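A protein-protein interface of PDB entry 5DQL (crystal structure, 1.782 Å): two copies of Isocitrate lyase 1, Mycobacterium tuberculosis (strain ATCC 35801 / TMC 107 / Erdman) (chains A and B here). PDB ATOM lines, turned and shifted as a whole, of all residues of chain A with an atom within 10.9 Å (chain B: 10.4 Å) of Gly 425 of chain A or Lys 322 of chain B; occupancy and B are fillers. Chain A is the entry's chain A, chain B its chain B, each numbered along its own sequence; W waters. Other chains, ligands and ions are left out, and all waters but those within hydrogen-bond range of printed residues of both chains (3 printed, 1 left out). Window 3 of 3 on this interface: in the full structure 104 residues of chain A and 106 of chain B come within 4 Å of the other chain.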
ATOM      1  N   VAL A 374      -7.959  22.333   2.871  1.00  0.00           N
ATOM      2  CA  VAL A 374      -7.392  21.785   1.649  1.00  0.00           C
ATOM      3  C   VAL A 374      -7.033  22.888   0.660  1.00  0.00           C
ATOM      4  O   VAL A 374      -6.024  22.790  -0.054  1.00  0.00           O
ATOM      5  CB  VAL A 374      -8.314  20.699   1.047  1.00  0.00           C
ATOM      6  CG1 VAL A 374      -7.874  20.328  -0.355  1.00  0.00           C
ATOM      7  CG2 VAL A 374      -8.308  19.480   1.945  1.00  0.00           C
ATOM      8  N   GLN A 377      -3.617  24.077   1.778  1.00  0.00           N
ATOM      9  CA  GLN A 377      -2.593  23.082   1.413  1.00  0.00           C
ATOM     10  C   GLN A 377      -2.314  23.100  -0.077  1.00  0.00           C
ATOM     11  O   GLN A 377      -1.152  23.013  -0.514  1.00  0.00           O
ATOM     12  CB  GLN A 377      -2.986  21.665   1.849  1.00  0.00           C
ATOM     13  CG  GLN A 377      -1.861  20.622   1.623  1.00  0.00           C
ATOM     14  CD  GLN A 377      -2.145  19.256   2.237  1.00  0.00           C
ATOM     15  OE1 GLN A 377      -3.120  18.576   1.872  1.00  0.00           O
ATOM     16  NE2 GLN A 377      -1.283  18.837   3.168  1.00  0.00           N
ATOM     17  N   GLU A 378      -3.379  23.221  -0.866  1.00  0.00           N
ATOM     18  CA  GLU A 378      -3.205  23.289  -2.310  1.00  0.00           C
ATOM     19  C   GLU A 378      -2.475  24.565  -2.731  1.00  0.00           C
ATOM     20  O   GLU A 378      -1.621  24.518  -3.615  1.00  0.00           O
ATOM     21  CB  GLU A 378      -4.539  23.098  -3.039  1.00  0.00           C
ATOM     22  CG  GLU A 378      -5.030  21.660  -2.986  1.00  0.00           C
ATOM     23  CD  GLU A 378      -4.033  20.686  -3.597  1.00  0.00           C
ATOM     24  OE1 GLU A 378      -3.506  20.988  -4.690  1.00  0.00           O
ATOM     25  OE2 GLU A 378      -3.767  19.626  -2.978  1.00  0.00           O
ATOM     26  N   PHE A 381       1.173  23.779  -1.997  1.00  0.00           N
ATOM     27  CA  PHE A 381       1.692  22.966  -3.092  1.00  0.00           C
ATOM     28  C   PHE A 381       2.028  23.854  -4.291  1.00  0.00           C
ATOM     29  O   PHE A 381       3.133  23.791  -4.831  1.00  0.00           O
ATOM     30  CB  PHE A 381       0.665  21.903  -3.490  1.00  0.00           C
ATOM     31  CG  PHE A 381       0.581  20.736  -2.536  1.00  0.00           C
ATOM     32  CD1 PHE A 381       1.733  20.155  -2.017  1.00  0.00           C
ATOM     33  CD2 PHE A 381      -0.654  20.217  -2.171  1.00  0.00           C
ATOM     34  CE1 PHE A 381       1.654  19.059  -1.149  1.00  0.00           C
ATOM     35  CE2 PHE A 381      -0.753  19.141  -1.298  1.00  0.00           C
ATOM     36  CZ  PHE A 381       0.410  18.561  -0.779  1.00  0.00           C
ATOM     37  N   LYS A 392       6.167  20.467   3.253  1.00  0.00           N
ATOM     38  CA  LYS A 392       6.835  19.363   3.938  1.00  0.00           C
ATOM     39  C   LYS A 392       7.285  19.847   5.305  1.00  0.00           C
ATOM     40  O   LYS A 392       8.454  20.164   5.504  1.00  0.00           O
ATOM     41  CB  LYS A 392       8.050  18.881   3.140  1.00  0.00           C
ATOM     42  CG  LYS A 392       7.707  18.380   1.719  1.00  0.00           C
ATOM     43  CD  LYS A 392       8.883  17.663   1.068  1.00  0.00           C
ATOM     44  CE  LYS A 392       8.585  17.300  -0.390  1.00  0.00           C
ATOM     45  NZ  LYS A 392       8.406  18.516  -1.242  1.00  0.00           N
ATOM     46  N   HIS A 393       6.357  19.907   6.251  1.00  0.00           N
ATOM     47  CA  HIS A 393       6.647  20.553   7.526  1.00  0.00           C
ATOM     48  C   HIS A 393       7.681  19.825   8.383  1.00  0.00           C
ATOM     49  O   HIS A 393       8.352  20.466   9.192  1.00  0.00           O
ATOM     50  CB  HIS A 393       5.359  20.782   8.317  1.00  0.00           C
ATOM     51  CG  HIS A 393       4.484  19.575   8.401  1.00  0.00           C
ATOM     52  ND1 HIS A 393       3.249  19.502   7.787  1.00  0.00           N
ATOM     53  CD2 HIS A 393       4.660  18.382   9.022  1.00  0.00           C
ATOM     54  CE1 HIS A 393       2.709  18.324   8.026  1.00  0.00           C
ATOM     55  NE2 HIS A 393       3.546  17.623   8.777  1.00  0.00           N
ATOM     56  N   GLN A 394       7.817  18.508   8.225  1.00  0.00           N
ATOM     57  CA  GLN A 394       8.778  17.767   9.061  1.00  0.00           C
ATOM     58  C   GLN A 394      10.214  18.185   8.768  1.00  0.00           C
ATOM     59  O   GLN A 394      10.962  18.540   9.674  1.00  0.00           O
ATOM     60  CB  GLN A 394       8.633  16.239   8.906  1.00  0.00           C
ATOM     61  CG  GLN A 394       7.198  15.669   9.017  1.00  0.00           C
ATOM     62  CD  GLN A 394       6.561  15.746  10.414  1.00  0.00           C
ATOM     63  OE1 GLN A 394       7.049  16.424  11.330  1.00  0.00           O
ATOM     64  NE2 GLN A 394       5.447  15.037  10.571  1.00  0.00           N
ATOM     65  N   ALA A 417      13.474   9.475  12.347  1.00  0.00           N
ATOM     66  CA  ALA A 417      12.139  10.044  12.150  1.00  0.00           C
ATOM     67  C   ALA A 417      11.592  10.061  10.721  1.00  0.00           C
ATOM     68  O   ALA A 417      10.416   9.774  10.503  1.00  0.00           O
ATOM     69  CB  ALA A 417      12.074  11.453  12.748  1.00  0.00           C
ATOM     70  N   LEU A 418      12.407  10.445   9.745  1.00  0.00           N
ATOM     71  CA  LEU A 418      11.855  10.648   8.403  1.00  0.00           C
ATOM     72  C   LEU A 418      11.508   9.336   7.665  1.00  0.00           C
ATOM     73  O   LEU A 418      10.488   9.257   6.966  1.00  0.00           O
ATOM     74  CB  LEU A 418      12.754  11.564   7.561  1.00  0.00           C
ATOM     75  CG  LEU A 418      12.728  13.066   7.865  1.00  0.00           C
ATOM     76  CD1 LEU A 418      13.534  13.831   6.826  1.00  0.00           C
ATOM     77  CD2 LEU A 418      11.311  13.597   7.896  1.00  0.00           C
ATOM     78  N   THR A 419      12.329   8.306   7.831  1.00  0.00           N
ATOM     79  CA  THR A 419      12.042   7.015   7.201  1.00  0.00           C
ATOM     80  C   THR A 419      10.758   6.407   7.765  1.00  0.00           C
ATOM     81  O   THR A 419      10.631   6.190   8.976  1.00  0.00           O
ATOM     82  CB  THR A 419      13.206   6.035   7.358  1.00  0.00           C
ATOM     83  OG1 THR A 419      14.342   6.559   6.663  1.00  0.00           O
ATOM     84  CG2 THR A 419      12.837   4.673   6.765  1.00  0.00           C
ATOM     85  N   GLY A 420       9.796   6.152   6.886  1.00  0.00           N
ATOM     86  CA  GLY A 420       8.529   5.579   7.307  1.00  0.00           C
ATOM     87  C   GLY A 420       7.487   6.633   7.649  1.00  0.00           C
ATOM     88  O   GLY A 420       6.352   6.297   7.984  1.00  0.00           O
ATOM     89  N   SER A 421       7.863   7.908   7.567  1.00  0.00           N
ATOM     90  CA  SER A 421       6.908   9.008   7.786  1.00  0.00           C
ATOM     91  C   SER A 421       5.919   9.192   6.618  1.00  0.00           C
ATOM     92  O   SER A 421       6.198   8.827   5.468  1.00  0.00           O
ATOM     93  CB  SER A 421       7.651  10.327   7.992  1.00  0.00           C
ATOM     94  OG  SER A 421       8.218  10.766   6.769  1.00  0.00           O
ATOM     95  N   THR A 422       4.760   9.761   6.919  1.00  0.00           N
ATOM     96  CA  THR A 422       3.810  10.107   5.874  1.00  0.00           C
ATOM     97  C   THR A 422       4.420  11.122   4.917  1.00  0.00           C
ATOM     98  O   THR A 422       4.119  11.115   3.728  1.00  0.00           O
ATOM     99  CB  THR A 422       2.495  10.659   6.444  1.00  0.00           C
ATOM    100  OG1 THR A 422       2.770  11.828   7.229  1.00  0.00           O
ATOM    101  CG2 THR A 422       1.802   9.607   7.309  1.00  0.00           C
ATOM    102  N   GLU A 423       5.295  11.982   5.424  1.00  0.00           N
ATOM    103  CA  GLU A 423       5.901  13.003   4.573  1.00  0.00           C
ATOM    104  C   GLU A 423       6.665  12.331   3.434  1.00  0.00           C
ATOM    105  O   GLU A 423       6.501  12.677   2.263  1.00  0.00           O
ATOM    106  CB  GLU A 423       6.839  13.901   5.364  1.00  0.00           C
ATOM    107  CG  GLU A 423       7.401  15.038   4.549  1.00  0.00           C
ATOM    108  CD  GLU A 423       7.900  16.170   5.432  1.00  0.00           C
ATOM    109  OE1 GLU A 423       7.052  16.909   5.988  1.00  0.00           O
ATOM    110  OE2 GLU A 423       9.134  16.298   5.591  1.00  0.00           O
ATOM    111  N   GLU A 424       7.506  11.378   3.801  1.00  0.00           N
ATOM    112  CA  GLU A 424       8.219  10.542   2.843  1.00  0.00           C
ATOM    113  C   GLU A 424       7.273   9.885   1.825  1.00  0.00           C
ATOM    114  O   GLU A 424       7.512   9.937   0.607  1.00  0.00           O
ATOM    115  CB  GLU A 424       9.005   9.472   3.604  1.00  0.00           C
ATOM    116  CG  GLU A 424       9.569   8.353   2.739  1.00  0.00           C
ATOM    117  CD  GLU A 424      10.515   7.458   3.517  1.00  0.00           C
ATOM    118  OE1 GLU A 424      10.042   6.463   4.126  1.00  0.00           O
ATOM    119  OE2 GLU A 424      11.730   7.767   3.530  1.00  0.00           O
ATOM    120  N   GLY A 425       6.194   9.285   2.323  1.00  0.00           N
ATOM    121  CA  GLY A 425       5.288   8.535   1.466  1.00  0.00           C
ATOM    122  C   GLY A 425       4.233   9.328   0.710  1.00  0.00           C
ATOM    123  O   GLY A 425       3.673   8.834  -0.268  1.00  0.00           O
ATOM    124  N   GLN A 426       3.946  10.554   1.136  1.00  0.00           N
ATOM    125  CA  GLN A 426       2.811  11.263   0.550  1.00  0.00           C
ATOM    126  C   GLN A 426       3.127  12.617  -0.088  1.00  0.00           C
ATOM    127  O   GLN A 426       2.295  13.170  -0.818  1.00  0.00           O
ATOM    128  CB  GLN A 426       1.694  11.424   1.589  1.00  0.00           C
ATOM    129  CG  GLN A 426       1.224  10.106   2.204  1.00  0.00           C
ATOM    130  CD  GLN A 426       0.019  10.288   3.105  1.00  0.00           C
ATOM    131  OE1 GLN A 426      -0.667  11.310   3.035  1.00  0.00           O
ATOM    132  NE2 GLN A 426      -0.248   9.297   3.956  1.00  0.00           N
ATOM    133  N   PHE A 427       4.320  13.145   0.178  1.00  0.00           N
ATOM    134  CA  PHE A 427       4.656  14.497  -0.264  1.00  0.00           C
ATOM    135  C   PHE A 427       5.819  14.569  -1.258  1.00  0.00           C
ATOM    136  O   PHE A 427       6.520  13.583  -1.489  1.00  0.00           O
ATOM    137  CB  PHE A 427       4.944  15.387   0.949  1.00  0.00           C
ATOM    138  CG  PHE A 427       3.731  15.700   1.775  1.00  0.00           C
ATOM    139  CD1 PHE A 427       3.128  14.723   2.557  1.00  0.00           C
ATOM    140  CD2 PHE A 427       3.208  16.987   1.793  1.00  0.00           C
ATOM    141  CE1 PHE A 427       2.007  15.016   3.330  1.00  0.00           C
ATOM    142  CE2 PHE A 427       2.084  17.293   2.560  1.00  0.00           C
ATOM    143  CZ  PHE A 427       1.480  16.306   3.331  1.00  0.00           C
ATOM    144  N   HIS B 193       2.822  10.898  12.817  1.00  0.00           N
ATOM    145  CA  HIS B 193       3.014  10.639  11.397  1.00  0.00           C
ATOM    146  C   HIS B 193       4.492  10.641  11.002  1.00  0.00           C
ATOM    147  O   HIS B 193       4.834  10.730   9.820  1.00  0.00           O
ATOM    148  CB  HIS B 193       2.176  11.609  10.562  1.00  0.00           C
ATOM    149  CG  HIS B 193       0.713  11.525  10.866  1.00  0.00           C
ATOM    150  ND1 HIS B 193       0.040  12.494  11.589  1.00  0.00           N
ATOM    151  CD2 HIS B 193      -0.199  10.558  10.604  1.00  0.00           C
ATOM    152  CE1 HIS B 193      -1.222  12.136  11.734  1.00  0.00           C
ATOM    153  NE2 HIS B 193      -1.396  10.963  11.144  1.00  0.00           N
ATOM    154  N   LEU B 194       5.360  10.553  12.009  1.00  0.00           N
ATOM    155  CA  LEU B 194       6.776  10.267  11.777  1.00  0.00           C
ATOM    156  C   LEU B 194       7.017   8.763  11.999  1.00  0.00           C
ATOM    157  O   LEU B 194       6.199   8.086  12.636  1.00  0.00           O
ATOM    158  CB  LEU B 194       7.666  11.126  12.695  1.00  0.00           C
ATOM    159  CG  LEU B 194       7.700  12.627  12.342  1.00  0.00           C
ATOM    160  CD1 LEU B 194       8.474  13.457  13.370  1.00  0.00           C
ATOM    161  CD2 LEU B 194       8.314  12.813  10.971  1.00  0.00           C
ATOM    162  N   GLY B 195       8.112   8.232  11.461  1.00  0.00           N
ATOM    163  CA  GLY B 195       8.485   6.842  11.733  1.00  0.00           C
ATOM    164  C   GLY B 195       9.357   6.768  12.981  1.00  0.00           C
ATOM    165  O   GLY B 195       9.563   7.776  13.657  1.00  0.00           O
ATOM    166  N   GLY B 287      -2.466   6.405   9.233  1.00  0.00           N
ATOM    167  CA  GLY B 287      -1.593   6.863   8.168  1.00  0.00           C
ATOM    168  C   GLY B 287      -2.263   7.613   7.033  1.00  0.00           C
ATOM    169  O   GLY B 287      -1.578   8.246   6.223  1.00  0.00           O
ATOM    170  N   THR B 288      -3.594   7.533   6.956  1.00  0.00           N
ATOM    171  CA  THR B 288      -4.360   8.236   5.922  1.00  0.00           C
ATOM    172  C   THR B 288      -5.708   8.728   6.445  1.00  0.00           C
ATOM    173  O   THR B 288      -6.259   8.171   7.404  1.00  0.00           O
ATOM    174  CB  THR B 288      -4.707   7.308   4.728  1.00  0.00           C
ATOM    175  OG1 THR B 288      -5.543   6.240   5.194  1.00  0.00           O
ATOM    176  CG2 THR B 288      -3.460   6.747   4.072  1.00  0.00           C
ATOM    177  N   PRO B 289      -6.259   9.762   5.798  1.00  0.00           N
ATOM    178  CA  PRO B 289      -7.632  10.154   6.123  1.00  0.00           C
ATOM    179  C   PRO B 289      -8.613   9.180   5.464  1.00  0.00           C
ATOM    180  O   PRO B 289      -8.884   9.270   4.261  1.00  0.00           O
ATOM    181  CB  PRO B 289      -7.747  11.555   5.518  1.00  0.00           C
ATOM    182  CG  PRO B 289      -6.754  11.568   4.395  1.00  0.00           C
ATOM    183  CD  PRO B 289      -5.627  10.666   4.820  1.00  0.00           C
ATOM    184  N   SER B 317      -0.308  16.395   7.959  1.00  0.00           N
ATOM    185  CA  SER B 317       0.685  15.399   7.547  1.00  0.00           C
ATOM    186  C   SER B 317       0.136  14.461   6.470  1.00  0.00           C
ATOM    187  O   SER B 317       0.853  13.595   5.972  1.00  0.00           O
ATOM    188  CB  SER B 317       1.192  14.583   8.746  1.00  0.00           C
ATOM    189  OG  SER B 317       1.836  15.428   9.689  1.00  0.00           O
ATOM    190  N   PHE B 318      -1.136  14.633   6.122  1.00  0.00           N
ATOM    191  CA  PHE B 318      -1.725  13.906   5.001  1.00  0.00           C
ATOM    192  C   PHE B 318      -1.719  14.797   3.772  1.00  0.00           C
ATOM    193  O   PHE B 318      -1.900  16.022   3.875  1.00  0.00           O
ATOM    194  CB  PHE B 318      -3.179  13.543   5.299  1.00  0.00           C
ATOM    195  CG  PHE B 318      -3.365  12.655   6.488  1.00  0.00           C
ATOM    196  CD1 PHE B 318      -2.431  11.678   6.806  1.00  0.00           C
ATOM    197  CD2 PHE B 318      -4.504  12.777   7.278  1.00  0.00           C
ATOM    198  CE1 PHE B 318      -2.624  10.847   7.885  1.00  0.00           C
ATOM    199  CE2 PHE B 318      -4.698  11.956   8.370  1.00  0.00           C
ATOM    200  CZ  PHE B 318      -3.757  10.982   8.677  1.00  0.00           C
ATOM    201  N   ASN B 319      -1.519  14.190   2.609  1.00  0.00           N
ATOM    202  CA  ASN B 319      -1.726  14.879   1.349  1.00  0.00           C
ATOM    203  C   ASN B 319      -3.185  14.632   0.990  1.00  0.00           C
ATOM    204  O   ASN B 319      -3.512  13.603   0.398  1.00  0.00           O
ATOM    205  CB  ASN B 319      -0.794  14.303   0.285  1.00  0.00           C
ATOM    206  CG  ASN B 319      -0.756  15.133  -0.980  1.00  0.00           C
ATOM    207  OD1 ASN B 319      -1.748  15.772  -1.356  1.00  0.00           O
ATOM    208  ND2 ASN B 319       0.388  15.118  -1.656  1.00  0.00           N
ATOM    209  N   TRP B 320      -4.063  15.551   1.385  1.00  0.00           N
ATOM    210  CA  TRP B 320      -5.505  15.308   1.309  1.00  0.00           C
ATOM    211  C   TRP B 320      -6.051  14.965  -0.083  1.00  0.00           C
ATOM    212  O   TRP B 320      -6.781  13.988  -0.234  1.00  0.00           O
ATOM    213  CB  TRP B 320      -6.293  16.445   1.976  1.00  0.00           C
ATOM    214  CG  TRP B 320      -6.105  16.403   3.452  1.00  0.00           C
ATOM    215  CD1 TRP B 320      -5.004  16.819   4.144  1.00  0.00           C
ATOM    216  CD2 TRP B 320      -7.004  15.856   4.421  1.00  0.00           C
ATOM    217  NE1 TRP B 320      -5.172  16.581   5.488  1.00  0.00           N
ATOM    218  CE2 TRP B 320      -6.398  15.992   5.687  1.00  0.00           C
ATOM    219  CE3 TRP B 320      -8.280  15.275   4.344  1.00  0.00           C
ATOM    220  CZ2 TRP B 320      -7.015  15.571   6.873  1.00  0.00           C
ATOM    221  CZ3 TRP B 320      -8.897  14.859   5.515  1.00  0.00           C
ATOM    222  CH2 TRP B 320      -8.263  15.005   6.766  1.00  0.00           C
ATOM    223  N   LYS B 321      -5.691  15.741  -1.097  1.00  0.00           N
ATOM    224  CA  LYS B 321      -6.271  15.517  -2.422  1.00  0.00           C
ATOM    225  C   LYS B 321      -5.589  14.383  -3.197  1.00  0.00           C
ATOM    226  O   LYS B 321      -6.070  13.964  -4.256  1.00  0.00           O
ATOM    227  CB  LYS B 321      -6.328  16.812  -3.236  1.00  0.00           C
ATOM    228  CG  LYS B 321      -7.500  17.711  -2.846  1.00  0.00           C
ATOM    229  CD  LYS B 321      -7.654  18.928  -3.758  1.00  0.00           C
ATOM    230  CE  LYS B 321      -8.162  18.556  -5.149  1.00  0.00           C
ATOM    231  NZ  LYS B 321      -7.031  18.335  -6.087  1.00  0.00           N
ATOM    232  N   LYS B 322      -4.484  13.874  -2.660  1.00  0.00           N
ATOM    233  CA  LYS B 322      -3.845  12.703  -3.238  1.00  0.00           C
ATOM    234  C   LYS B 322      -4.661  11.484  -2.850  1.00  0.00           C
ATOM    235  O   LYS B 322      -4.682  10.477  -3.560  1.00  0.00           O
ATOM    236  CB  LYS B 322      -2.415  12.549  -2.720  1.00  0.00           C
ATOM    237  CG  LYS B 322      -1.663  11.392  -3.348  1.00  0.00           C
ATOM    238  CD  LYS B 322      -0.459  10.992  -2.511  1.00  0.00           C
ATOM    239  CE  LYS B 322       0.194   9.722  -3.053  1.00  0.00           C
ATOM    240  NZ  LYS B 322       1.011   9.042  -1.999  1.00  0.00           N
ATOM    241  N   HIS B 323      -5.345  11.586  -1.715  1.00  0.00           N
ATOM    242  CA  HIS B 323      -6.078  10.449  -1.166  1.00  0.00           C
ATOM    243  C   HIS B 323      -7.599  10.519  -1.336  1.00  0.00           C
ATOM    244  O   HIS B 323      -8.255   9.480  -1.383  1.00  0.00           O
ATOM    245  CB  HIS B 323      -5.710  10.242   0.304  1.00  0.00           C
ATOM    246  CG  HIS B 323      -4.259   9.957   0.520  1.00  0.00           C
ATOM    247  ND1 HIS B 323      -3.658   8.781   0.104  1.00  0.00           N
ATOM    248  CD2 HIS B 323      -3.274  10.692   1.093  1.00  0.00           C
ATOM    249  CE1 HIS B 323      -2.378   8.807   0.413  1.00  0.00           C
ATOM    250  NE2 HIS B 323      -2.116   9.958   1.015  1.00  0.00           N
ATOM    251  N   LEU B 324      -8.157  11.728  -1.426  1.00  0.00           N
ATOM    252  CA  LEU B 324      -9.620  11.886  -1.488  1.00  0.00           C
ATOM    253  C   LEU B 324     -10.094  12.845  -2.591  1.00  0.00           C
ATOM    254  O   LEU B 324      -9.341  13.720  -3.034  1.00  0.00           O
ATOM    255  CB  LEU B 324     -10.173  12.352  -0.138  1.00  0.00           C
ATOM    256  CG  LEU B 324      -9.746  11.627   1.142  1.00  0.00           C
ATOM    257  CD1 LEU B 324     -10.148  12.435   2.371  1.00  0.00           C
ATOM    258  CD2 LEU B 324     -10.323  10.220   1.231  1.00  0.00           C
ATOM    259  N   ASP B 325     -11.344  12.683  -3.028  1.00  0.00           N
ATOM    260  CA  ASP B 325     -11.957  13.644  -3.953  1.00  0.00           C
ATOM    261  C   ASP B 325     -12.644  14.769  -3.171  1.00  0.00           C
ATOM    262  O   ASP B 325     -12.987  14.583  -1.997  1.00  0.00           O
ATOM    263  CB  ASP B 325     -12.936  12.956  -4.925  1.00  0.00           C
ATOM    264  CG  ASP B 325     -14.004  12.121  -4.216  1.00  0.00           C
ATOM    265  OD1 ASP B 325     -14.565  12.570  -3.198  1.00  0.00           O
ATOM    266  OD2 ASP B 325     -14.305  11.001  -4.694  1.00  0.00           O
ATOM    267  N   ASP B 326     -12.845  15.920  -3.820  1.00  0.00           N
ATOM    268  CA  ASP B 326     -13.413  17.097  -3.150  1.00  0.00           C
ATOM    269  C   ASP B 326     -14.751  16.790  -2.474  1.00  0.00           C
ATOM    270  O   ASP B 326     -15.074  17.347  -1.429  1.00  0.00           O
ATOM    271  CB  ASP B 326     -13.565  18.269  -4.128  1.00  0.00           C
ATOM    272  CG  ASP B 326     -12.236  18.805  -4.619  1.00  0.00           C
ATOM    273  OD1 ASP B 326     -11.220  18.653  -3.913  1.00  0.00           O
ATOM    274  OD2 ASP B 326     -12.203  19.387  -5.723  1.00  0.00           O
ATOM    275  N   THR B 328     -15.579  13.948  -0.990  1.00  0.00           N
ATOM    276  CA  THR B 328     -15.305  13.233   0.260  1.00  0.00           C
ATOM    277  C   THR B 328     -14.641  14.157   1.284  1.00  0.00           C
ATOM    278  O   THR B 328     -14.893  14.047   2.485  1.00  0.00           O
ATOM    279  CB  THR B 328     -14.367  12.015   0.054  1.00  0.00           C
ATOM    280  OG1 THR B 328     -14.724  11.304  -1.142  1.00  0.00           O
ATOM    281  CG2 THR B 328     -14.445  11.086   1.257  1.00  0.00           C
ATOM    282  N   ILE B 329     -13.788  15.055   0.803  1.00  0.00           N
ATOM    283  CA  ILE B 329     -13.177  16.058   1.682  1.00  0.00           C
ATOM    284  C   ILE B 329     -14.269  16.947   2.307  1.00  0.00           C
ATOM    285  O   ILE B 329     -14.272  17.179   3.515  1.00  0.00           O
ATOM    286  CB  ILE B 329     -12.094  16.865   0.933  1.00  0.00           C
ATOM    287  CG1 ILE B 329     -10.866  15.977   0.678  1.00  0.00           C
ATOM    288  CG2 ILE B 329     -11.696  18.127   1.714  1.00  0.00           C
ATOM    289  CD1 ILE B 329      -9.894  16.517  -0.381  1.00  0.00           C
HETATM  290  O   HOH W   1       4.879  13.093   8.308  1.00  0.00           O
HETATM  291  O   HOH W   2      -4.489  18.478  -0.893  1.00  0.00           O
HETATM  292  O   HOH W   3       3.560  14.732   6.552  1.00  0.00           O
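The side-chain amide oxygen (OE1) of Gln 426 of chain A is in hydrogen-bond range of a ring nitrogen (NE2) of His 323 of chain B (2.8 Å). The side-chain amide nitrogen (ND2) of Asn 319 of chain B lies within hydrogen-bond range of the backbone carbonyl oxygen (O) of Gln 426 of chain A (2.9 Å). The side-chain amide oxygen (OE1) of Gln 377 of chain A lies within hydrogen-bond range of the backbone NH (N) of Trp 320 of chain B (3.2 Å). NE2 of Gln 426 of chain A lies within hydrogen-bond range of O of Gly 287 of chain B. The backbone carbonyl oxygen of Gly 425 of chain A lies within hydrogen-bond range of the side-chain amino group of Lys 322 of chain B (3.2 Å). The backbone carbonyl oxygen of Phe 318 of chain B is in hydrogen-bond range of the side-chain amide nitrogen of Gln 377 of chain A, 3.0 Å away. N of Thr 422 of chain A sits at hydrogen-bond distance from O of His 193 of chain B. O of Ala 417 of chain A sits at hydrogen-bond distance from N of Gly 195 of chain B. OG1 of Thr 422 of chain A sits at hydrogen-bond distance from O of Ser 317 of chain B, 2.9 Å away. The side-chain hydroxyl (OG) of Ser 317 of chain B lies within hydrogen-bond range of a ring nitrogen (NE2) of His 393 of chain A (2.9 Å).
Printed residues of chain B within 4 Å of Val 374 of chain A: Trp 320, Lys 321 and Ile 329. Of the printed residues of chain B, Ser 421 of chain A touches His 193 (3.4 Å), Leu 194 (3.9 Å) and Gly 195 (3.9 Å). No residue of chain B comes within 4 Å of Glu 424 of chain A. Gly 425 of chain A touches just one residue of chain B: Lys 322. Pro 289 of chain B touches none of the printed residues of chain A. Printed residues of chain A within 4 Å of Lys 321 of chain B: Val 374 and Glu 378. Leu 324 of chain B touches none of the printed residues of chain A. The nearest residue of chain A that does not touch Lys 322 of chain B is Phe 427 of chain A (5.7 Å).
O of Leu 418 of chain A is in hydrogen-bond range of OG of Ser 421 of chain A (2.7 Å). The side-chain carboxylate of Glu 423 of chain A lies within hydrogen-bond range of the backbone NH of Gln 394 of chain A (2.9 Å). OG of Ser 421 of chain A lies within hydrogen-bond range of N of Glu 424 of chain A (3.1 Å).
Among the printed residues, pairs that only touch across the chains: Phe 427 of chain A with Ser 317 of chain B (3.2 Å), Ser 421 of chain A with His 193 of chain B (3.4 Å), Gln 426 of chain A with Phe 318 of chain B (3.4 Å), Phe 427 of chain A with Phe 318 of chain B (3.4 Å), Gln 394 of chain A with Leu 194 of chain B (3.5 Å), Phe 381 of chain A with Asn 319 of chain B (3.5 Å), Thr 419 of chain A with Gly 195 of chain B (3.6 Å), Val 374 of chain A with Lys 321 of chain B (3.6 Å), Val 374 of chain A with Trp 320 of chain B (3.6 Å), Val 374 of chain A with Ile 329 of chain B (3.7 Å), Phe 427 of chain A with Asn 319 of chain B (3.7 Å), Ala 417 of chain A with Leu 194 of chain B (3.7 Å), Gln 394 of chain A with Ser 317 of chain B (3.7 Å), Thr 422 of chain A with Gly 287 of chain B (3.8 Å), Glu 378 of chain A with Lys 321 of chain B (3.8 Å), Gln 426 of chain A with Lys 322 of chain B (3.8 Å), Ser 421 of chain A with Leu 194 of chain B (3.9 Å), Ser 421 of chain A with Gly 195 of chain B (3.9 Å) and Gln 377 of chain A with Asn 319 of chain B (3.99 Å).
Water W1 lies within hydrogen-bond range of OG1 of Thr 422 of chain A (2.7 Å), O of His 193 of chain B (2.8 Å), NE2 of Gln 394 of chain A (3.0 Å) and N of Glu 423 of chain A (3.1 Å). Water W3 lies within hydrogen-bond range of O of Ser 317 of chain B (3.0 Å), OG1 of Thr 422 of chain A (3.1 Å) and N of Glu 423 of chain A (3.4 Å).
No position is printed for both chains. Of the 29 pairs that touch across the chains among the printed residues, none has its exchanged pair printed and touching as well.
Of the 18 printed residues of chain B, 12 touch a printed residue of chain A. Printed residues of chain B that touch a printed residue of chain A: His 193, Leu 194, Gly 195, Gly 287, Ser 317, Phe 318, Asn 319, Trp 320, Lys 321, Lys 322, His 323 and Ile 329. Of the 18 printed residues of chain A, 13 touch a printed residue of chain B. Hydrophobic or aromatic side chains of chain A that line the printed part of chain B: Val 374, Phe 381, His 393 and Phe 427.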
